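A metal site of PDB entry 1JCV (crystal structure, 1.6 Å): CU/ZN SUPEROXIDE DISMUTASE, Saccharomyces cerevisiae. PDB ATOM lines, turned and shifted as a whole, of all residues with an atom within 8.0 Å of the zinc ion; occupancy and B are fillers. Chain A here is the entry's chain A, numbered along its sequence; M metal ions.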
ATOM      1  N   PHE A  45      21.122  -8.623 -11.546  1.00  0.00           N
ATOM      2  CA  PHE A  45      20.615  -7.471 -12.298  1.00  0.00           C
ATOM      3  C   PHE A  45      21.761  -6.453 -12.405  1.00  0.00           C
ATOM      4  O   PHE A  45      22.278  -5.982 -11.385  1.00  0.00           O
ATOM      5  CB  PHE A  45      19.459  -6.921 -11.449  1.00  0.00           C
ATOM      6  CG  PHE A  45      18.661  -5.820 -12.088  1.00  0.00           C
ATOM      7  CD1 PHE A  45      18.146  -5.951 -13.374  1.00  0.00           C
ATOM      8  CD2 PHE A  45      18.346  -4.678 -11.366  1.00  0.00           C
ATOM      9  CE1 PHE A  45      17.331  -4.946 -13.921  1.00  0.00           C
ATOM     10  CE2 PHE A  45      17.539  -3.667 -11.900  1.00  0.00           C
ATOM     11  CZ  PHE A  45      17.031  -3.810 -13.183  1.00  0.00           C
ATOM     12  N   HIS A  46      22.222  -6.140 -13.611  1.00  0.00           N
ATOM     13  CA  HIS A  46      23.345  -5.204 -13.737  1.00  0.00           C
ATOM     14  C   HIS A  46      23.328  -4.376 -15.002  1.00  0.00           C
ATOM     15  O   HIS A  46      22.634  -4.704 -15.971  1.00  0.00           O
ATOM     16  CB  HIS A  46      24.701  -5.924 -13.754  1.00  0.00           C
ATOM     17  CG  HIS A  46      24.754  -7.179 -12.952  1.00  0.00           C
ATOM     18  ND1 HIS A  46      24.709  -8.435 -13.529  1.00  0.00           N
ATOM     19  CD2 HIS A  46      24.831  -7.376 -11.618  1.00  0.00           C
ATOM     20  CE1 HIS A  46      24.739  -9.348 -12.580  1.00  0.00           C
ATOM     21  NE2 HIS A  46      24.815  -8.733 -11.410  1.00  0.00           N
ATOM     22  N   ILE A  47      24.161  -3.343 -15.008  1.00  0.00           N
ATOM     23  CA  ILE A  47      24.357  -2.531 -16.181  1.00  0.00           C
ATOM     24  C   ILE A  47      25.661  -3.063 -16.798  1.00  0.00           C
ATOM     25  O   ILE A  47      26.648  -3.264 -16.098  1.00  0.00           O
ATOM     26  CB  ILE A  47      24.475  -1.051 -15.818  1.00  0.00           C
ATOM     27  CG1 ILE A  47      23.104  -0.583 -15.306  1.00  0.00           C
ATOM     28  CG2 ILE A  47      24.899  -0.242 -17.044  1.00  0.00           C
ATOM     29  CD1 ILE A  47      23.093   0.797 -14.731  1.00  0.00           C
ATOM     30  N   HIS A  48      25.574  -3.445 -18.075  1.00  0.00           N
ATOM     31  CA  HIS A  48      26.713  -3.965 -18.814  1.00  0.00           C
ATOM     32  C   HIS A  48      27.290  -2.849 -19.664  1.00  0.00           C
ATOM     33  O   HIS A  48      26.577  -1.888 -20.003  1.00  0.00           O
ATOM     34  CB  HIS A  48      26.320  -5.201 -19.631  1.00  0.00           C
ATOM     35  CG  HIS A  48      26.133  -6.432 -18.810  1.00  0.00           C
ATOM     36  ND1 HIS A  48      26.793  -7.610 -19.068  1.00  0.00           N
ATOM     37  CD2 HIS A  48      25.387  -6.655 -17.698  1.00  0.00           C
ATOM     38  CE1 HIS A  48      26.477  -8.511 -18.156  1.00  0.00           C
ATOM     39  NE2 HIS A  48      25.615  -7.960 -17.305  1.00  0.00           N
ATOM     40  N   PRO A  62      30.743  -7.146 -20.668  1.00  0.00           N
ATOM     41  CA  PRO A  62      30.856  -7.369 -19.227  1.00  0.00           C
ATOM     42  C   PRO A  62      30.137  -6.320 -18.381  1.00  0.00           C
ATOM     43  O   PRO A  62      29.544  -5.392 -18.927  1.00  0.00           O
ATOM     44  CB  PRO A  62      32.369  -7.297 -19.019  1.00  0.00           C
ATOM     45  CG  PRO A  62      32.742  -6.183 -19.950  1.00  0.00           C
ATOM     46  CD  PRO A  62      31.964  -6.521 -21.205  1.00  0.00           C
ATOM     47  N   HIS A  63      30.168  -6.472 -17.064  1.00  0.00           N
ATOM     48  CA  HIS A  63      29.547  -5.501 -16.177  1.00  0.00           C
ATOM     49  C   HIS A  63      30.282  -4.177 -16.385  1.00  0.00           C
ATOM     50  O   HIS A  63      31.505  -4.175 -16.579  1.00  0.00           O
ATOM     51  CB  HIS A  63      29.678  -5.929 -14.711  1.00  0.00           C
ATOM     52  CG  HIS A  63      28.941  -7.185 -14.398  1.00  0.00           C
ATOM     53  ND1 HIS A  63      28.810  -7.673 -13.117  1.00  0.00           N
ATOM     54  CD2 HIS A  63      28.274  -8.035 -15.202  1.00  0.00           C
ATOM     55  CE1 HIS A  63      28.100  -8.788 -13.153  1.00  0.00           C
ATOM     56  NE2 HIS A  63      27.759  -9.032 -14.407  1.00  0.00           N
ATOM     57  N   PHE A  64      29.540  -3.079 -16.395  1.00  0.00           N
ATOM     58  CA  PHE A  64      30.144  -1.762 -16.578  1.00  0.00           C
ATOM     59  C   PHE A  64      31.043  -1.544 -15.352  1.00  0.00           C
ATOM     60  O   PHE A  64      30.573  -1.564 -14.204  1.00  0.00           O
ATOM     61  CB  PHE A  64      29.049  -0.703 -16.704  1.00  0.00           C
ATOM     62  CG  PHE A  64      29.568   0.688 -16.897  1.00  0.00           C
ATOM     63  CD1 PHE A  64      30.633   0.927 -17.748  1.00  0.00           C
ATOM     64  CD2 PHE A  64      28.970   1.766 -16.232  1.00  0.00           C
ATOM     65  CE1 PHE A  64      31.110   2.226 -17.924  1.00  0.00           C
ATOM     66  CE2 PHE A  64      29.434   3.068 -16.402  1.00  0.00           C
ATOM     67  CZ  PHE A  64      30.511   3.306 -17.245  1.00  0.00           C
ATOM     68  N   ASN A  65      32.336  -1.355 -15.610  1.00  0.00           N
ATOM     69  CA  ASN A  65      33.328  -1.248 -14.547  1.00  0.00           C
ATOM     70  C   ASN A  65      34.470  -0.304 -14.945  1.00  0.00           C
ATOM     71  O   ASN A  65      35.632  -0.721 -15.038  1.00  0.00           O
ATOM     72  CB  ASN A  65      33.869  -2.671 -14.319  1.00  0.00           C
ATOM     73  CG  ASN A  65      34.858  -2.773 -13.189  1.00  0.00           C
ATOM     74  OD1 ASN A  65      34.827  -1.974 -12.249  1.00  0.00           O
ATOM     75  ND2 ASN A  65      35.688  -3.801 -13.225  1.00  0.00           N
ATOM     76  N   LYS A  69      37.168  -2.299 -10.565  1.00  0.00           N
ATOM     77  CA  LYS A  69      37.003  -2.872  -9.252  1.00  0.00           C
ATOM     78  C   LYS A  69      36.453  -4.287  -9.431  1.00  0.00           C
ATOM     79  O   LYS A  69      36.100  -4.680 -10.542  1.00  0.00           O
ATOM     80  CB  LYS A  69      36.001  -2.014  -8.445  1.00  0.00           C
ATOM     81  CG  LYS A  69      36.355  -0.508  -8.303  1.00  0.00           C
ATOM     82  CD  LYS A  69      37.647  -0.280  -7.520  1.00  0.00           C
ATOM     83  CE  LYS A  69      37.976   1.209  -7.270  1.00  0.00           C
ATOM     84  NZ  LYS A  69      38.852   1.891  -8.332  1.00  0.00           N
ATOM     85  N   THR A  70      36.411  -5.067  -8.350  1.00  0.00           N
ATOM     86  CA  THR A  70      35.843  -6.406  -8.427  1.00  0.00           C
ATOM     87  C   THR A  70      34.323  -6.296  -8.261  1.00  0.00           C
ATOM     88  O   THR A  70      33.802  -5.297  -7.757  1.00  0.00           O
ATOM     89  CB  THR A  70      36.370  -7.362  -7.337  1.00  0.00           C
ATOM     90  OG1 THR A  70      36.264  -6.724  -6.057  1.00  0.00           O
ATOM     91  CG2 THR A  70      37.831  -7.786  -7.619  1.00  0.00           C
ATOM     92  N   HIS A  71      33.633  -7.359  -8.676  1.00  0.00           N
ATOM     93  CA  HIS A  71      32.178  -7.456  -8.588  1.00  0.00           C
ATOM     94  C   HIS A  71      31.757  -7.527  -7.121  1.00  0.00           C
ATOM     95  O   HIS A  71      32.362  -8.265  -6.337  1.00  0.00           O
ATOM     96  CB  HIS A  71      31.737  -8.732  -9.317  1.00  0.00           C
ATOM     97  CG  HIS A  71      30.277  -8.990  -9.206  1.00  0.00           C
ATOM     98  ND1 HIS A  71      29.352  -8.351  -9.994  1.00  0.00           N
ATOM     99  CD2 HIS A  71      29.576  -9.765  -8.345  1.00  0.00           C
ATOM    100  CE1 HIS A  71      28.133  -8.703  -9.605  1.00  0.00           C
ATOM    101  NE2 HIS A  71      28.252  -9.552  -8.608  1.00  0.00           N
ATOM    102  N   GLY A  72      30.706  -6.787  -6.751  1.00  0.00           N
ATOM    103  CA  GLY A  72      30.229  -6.793  -5.384  1.00  0.00           C
ATOM    104  C   GLY A  72      28.743  -6.511  -5.269  1.00  0.00           C
ATOM    105  O   GLY A  72      28.016  -6.545  -6.264  1.00  0.00           O
ATOM    106  N   ALA A  73      28.284  -6.339  -4.042  1.00  0.00           N
ATOM    107  CA  ALA A  73      26.884  -6.008  -3.776  1.00  0.00           C
ATOM    108  C   ALA A  73      26.757  -4.488  -3.970  1.00  0.00           C
ATOM    109  O   ALA A  73      27.728  -3.759  -3.870  1.00  0.00           O
ATOM    110  CB  ALA A  73      26.537  -6.386  -2.343  1.00  0.00           C
ATOM    111  N   ARG A  79      32.784  -2.434  -5.772  1.00  0.00           N
ATOM    112  CA  ARG A  79      31.814  -3.033  -6.674  1.00  0.00           C
ATOM    113  C   ARG A  79      32.009  -2.410  -8.063  1.00  0.00           C
ATOM    114  O   ARG A  79      32.775  -1.442  -8.223  1.00  0.00           O
ATOM    115  CB  ARG A  79      30.384  -2.753  -6.210  1.00  0.00           C
ATOM    116  CG  ARG A  79      30.072  -1.271  -6.048  1.00  0.00           C
ATOM    117  CD  ARG A  79      28.606  -0.986  -5.803  1.00  0.00           C
ATOM    118  NE  ARG A  79      27.947  -0.633  -7.043  1.00  0.00           N
ATOM    119  CZ  ARG A  79      26.870   0.138  -7.111  1.00  0.00           C
ATOM    120  NH1 ARG A  79      26.325   0.601  -5.991  1.00  0.00           N
ATOM    121  NH2 ARG A  79      26.383   0.509  -8.311  1.00  0.00           N
ATOM    122  N   HIS A  80      31.364  -3.001  -9.054  1.00  0.00           N
ATOM    123  CA  HIS A  80      31.397  -2.458 -10.416  1.00  0.00           C
ATOM    124  C   HIS A  80      30.329  -1.364 -10.395  1.00  0.00           C
ATOM    125  O   HIS A  80      29.350  -1.465  -9.658  1.00  0.00           O
ATOM    126  CB  HIS A  80      30.961  -3.527 -11.434  1.00  0.00           C
ATOM    127  CG  HIS A  80      31.912  -4.677 -11.549  1.00  0.00           C
ATOM    128  ND1 HIS A  80      31.509  -5.962 -11.879  1.00  0.00           N
ATOM    129  CD2 HIS A  80      33.260  -4.721 -11.446  1.00  0.00           C
ATOM    130  CE1 HIS A  80      32.576  -6.733 -11.992  1.00  0.00           C
ATOM    131  NE2 HIS A  80      33.650  -6.007 -11.731  1.00  0.00           N
ATOM    132  N   VAL A  81      30.523  -0.297 -11.162  1.00  0.00           N
ATOM    133  CA  VAL A  81      29.507   0.743 -11.229  1.00  0.00           C
ATOM    134  C   VAL A  81      28.149   0.104 -11.562  1.00  0.00           C
ATOM    135  O   VAL A  81      27.124   0.452 -10.981  1.00  0.00           O
ATOM    136  CB  VAL A  81      29.864   1.784 -12.323  1.00  0.00           C
ATOM    137  CG1 VAL A  81      28.637   2.646 -12.690  1.00  0.00           C
ATOM    138  CG2 VAL A  81      31.054   2.653 -11.852  1.00  0.00           C
ATOM    139  N   GLY A  82      28.155  -0.859 -12.487  1.00  0.00           N
ATOM    140  CA  GLY A  82      26.906  -1.490 -12.912  1.00  0.00           C
ATOM    141  C   GLY A  82      26.236  -2.516 -12.011  1.00  0.00           C
ATOM    142  O   GLY A  82      25.172  -3.026 -12.360  1.00  0.00           O
ATOM    143  N   ASP A  83      26.824  -2.819 -10.863  1.00  0.00           N
ATOM    144  CA  ASP A  83      26.273  -3.814  -9.957  1.00  0.00           C
ATOM    145  C   ASP A  83      25.003  -3.390  -9.236  1.00  0.00           C
ATOM    146  O   ASP A  83      25.021  -2.513  -8.361  1.00  0.00           O
ATOM    147  CB  ASP A  83      27.336  -4.265  -8.948  1.00  0.00           C
ATOM    148  CG  ASP A  83      28.454  -5.086  -9.587  1.00  0.00           C
ATOM    149  OD1 ASP A  83      28.293  -5.587 -10.731  1.00  0.00           O
ATOM    150  OD2 ASP A  83      29.519  -5.263  -8.970  1.00  0.00           O
ATOM    151  N   MET A  84      23.887  -3.993  -9.626  1.00  0.00           N
ATOM    152  CA  MET A  84      22.588  -3.726  -9.005  1.00  0.00           C
ATOM    153  C   MET A  84      22.094  -4.933  -8.178  1.00  0.00           C
ATOM    154  O   MET A  84      20.920  -5.006  -7.812  1.00  0.00           O
ATOM    155  CB  MET A  84      21.572  -3.299 -10.057  1.00  0.00           C
ATOM    156  CG  MET A  84      22.042  -2.090 -10.851  1.00  0.00           C
ATOM    157  SD  MET A  84      20.757  -1.391 -11.901  1.00  0.00           S
ATOM    158  CE  MET A  84      20.664  -2.613 -13.225  1.00  0.00           C
ATOM    159  N   GLY A  85      22.996  -5.865  -7.871  1.00  0.00           N
ATOM    160  CA  GLY A  85      22.653  -7.016  -7.046  1.00  0.00           C
ATOM    161  C   GLY A  85      21.608  -7.965  -7.616  1.00  0.00           C
ATOM    162  O   GLY A  85      21.673  -8.335  -8.789  1.00  0.00           O
ATOM    163  N   ASP A 124      22.933 -13.781  -8.074  1.00  0.00           N
ATOM    164  CA  ASP A 124      24.227 -13.126  -8.028  1.00  0.00           C
ATOM    165  C   ASP A 124      24.767 -13.406  -6.629  1.00  0.00           C
ATOM    166  O   ASP A 124      24.091 -13.099  -5.662  1.00  0.00           O
ATOM    167  CB  ASP A 124      23.992 -11.617  -8.230  1.00  0.00           C
ATOM    168  CG  ASP A 124      25.275 -10.792  -8.282  1.00  0.00           C
ATOM    169  OD1 ASP A 124      26.309 -11.207  -7.719  1.00  0.00           O
ATOM    170  OD2 ASP A 124      25.227  -9.696  -8.866  1.00  0.00           O
ATOM    171  N   LEU A 126      27.113 -11.949  -5.189  1.00  0.00           N
ATOM    172  CA  LEU A 126      27.617 -10.685  -4.697  1.00  0.00           C
ATOM    173  C   LEU A 126      29.129 -10.610  -4.511  1.00  0.00           C
ATOM    174  O   LEU A 126      29.626  -9.761  -3.750  1.00  0.00           O
ATOM    175  CB  LEU A 126      26.859 -10.290  -3.427  1.00  0.00           C
ATOM    176  CG  LEU A 126      25.324 -10.382  -3.555  1.00  0.00           C
ATOM    177  CD1 LEU A 126      24.667 -10.007  -2.245  1.00  0.00           C
ATOM    178  CD2 LEU A 126      24.800  -9.474  -4.688  1.00  0.00           C
ATOM    179  N   GLY A 127      29.849 -11.429  -5.262  1.00  0.00           N
ATOM    180  CA  GLY A 127      31.303 -11.438  -5.184  1.00  0.00           C
ATOM    181  C   GLY A 127      31.800 -12.147  -3.954  1.00  0.00           C
ATOM    182  O   GLY A 127      32.979 -12.087  -3.643  1.00  0.00           O
ATOM    183  N   SER A 134      33.398 -15.353  -9.226  1.00  0.00           N
ATOM    184  CA  SER A 134      32.520 -14.623  -8.331  1.00  0.00           C
ATOM    185  C   SER A 134      32.866 -13.143  -8.387  1.00  0.00           C
ATOM    186  O   SER A 134      31.980 -12.285  -8.366  1.00  0.00           O
ATOM    187  CB  SER A 134      32.688 -15.120  -6.909  1.00  0.00           C
ATOM    188  OG  SER A 134      31.867 -14.369  -6.020  1.00  0.00           O
ATOM    189  N   LEU A 135      34.165 -12.859  -8.465  1.00  0.00           N
ATOM    190  CA  LEU A 135      34.662 -11.493  -8.520  1.00  0.00           C
ATOM    191  C   LEU A 135      34.504 -10.823  -9.874  1.00  0.00           C
ATOM    192  O   LEU A 135      34.831  -9.648 -10.029  1.00  0.00           O
ATOM    193  CB  LEU A 135      36.119 -11.446  -8.076  1.00  0.00           C
ATOM    194  CG  LEU A 135      36.395 -11.933  -6.647  1.00  0.00           C
ATOM    195  CD1 LEU A 135      37.891 -11.894  -6.392  1.00  0.00           C
ATOM    196  CD2 LEU A 135      35.648 -11.087  -5.637  1.00  0.00           C
ATOM    197  N   LYS A 136      33.971 -11.562 -10.848  1.00  0.00           N
ATOM    198  CA  LYS A 136      33.751 -11.010 -12.182  1.00  0.00           C
ATOM    199  C   LYS A 136      32.277 -10.814 -12.541  1.00  0.00           C
ATOM    200  O   LYS A 136      31.869  -9.723 -12.960  1.00  0.00           O
ATOM    201  CB  LYS A 136      34.352 -11.922 -13.259  1.00  0.00           C
ATOM    202  CG  LYS A 136      35.832 -12.128 -13.178  1.00  0.00           C
ATOM    203  CD  LYS A 136      36.273 -12.887 -14.412  1.00  0.00           C
ATOM    204  CE  LYS A 136      37.703 -13.384 -14.313  1.00  0.00           C
ATOM    205  NZ  LYS A 136      38.160 -13.851 -15.676  1.00  0.00           N
ATOM    206  N   THR A 137      31.494 -11.877 -12.362  1.00  0.00           N
ATOM    207  CA  THR A 137      30.085 -11.866 -12.724  1.00  0.00           C
ATOM    208  C   THR A 137      29.159 -12.198 -11.560  1.00  0.00           C
ATOM    209  O   THR A 137      27.954 -12.102 -11.703  1.00  0.00           O
ATOM    210  CB  THR A 137      29.817 -12.952 -13.782  1.00  0.00           C
ATOM    211  OG1 THR A 137      30.092 -14.241 -13.223  1.00  0.00           O
ATOM    212  CG2 THR A 137      30.696 -12.766 -14.985  1.00  0.00           C
ATOM    213  N   GLY A 138      29.715 -12.590 -10.408  1.00  0.00           N
ATOM    214  CA  GLY A 138      28.890 -12.964  -9.280  1.00  0.00           C
ATOM    215  C   GLY A 138      28.221 -14.304  -9.545  1.00  0.00           C
ATOM    216  O   GLY A 138      27.286 -14.680  -8.835  1.00  0.00           O
HETATM  217 ZN    ZN M   1      29.578  -6.827 -11.429  1.00  0.00          ZN
HETATM  218 CU    CU M   2      24.834  -8.826 -15.606  1.00  0.00          CU
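Lys 136 touches the zinc ion (O to ZN, 3.997 Å). Of the 28 residues printed, 5 come within 4 Å of the zinc ion. The nearest printed residue that does not touch the zinc ion is His 46 (4.8 Å).
The zinc ion is bound by OD1 of Asp 83 (1.9 Å), ND1 of His 63 (2.0 Å), ND1 of His 71 (2.1 Å) and ND1 of His 80 (2.2 Å).
The side-chain carboxylate (OD2) of Asp 83 sits at hydrogen-bond distance from the backbone NH (N) of Gly 72, 2.9 Å away. A ring nitrogen (NE2) of His 71 is in hydrogen-bond range of the side-chain carboxylate (OD1) of Asp 124 (2.7 Å). N of His 71 lies within hydrogen-bond range of O of Leu 135, 2.9 Å away. NE2 of His 80 lies close to O of Lys 69. The side-chain amide nitrogen (ND2) of Asn 65 lies close to a ring nitrogen (NE2) of His 80 (3.4 Å). NE2 of His 63 sits close to ND1 of His 46 (3.2 Å). The guanidinium group (NH2) of Arg 79 lies within hydrogen-bond range of the backbone carbonyl oxygen (O) of Asp 83, 3.3 Å away.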
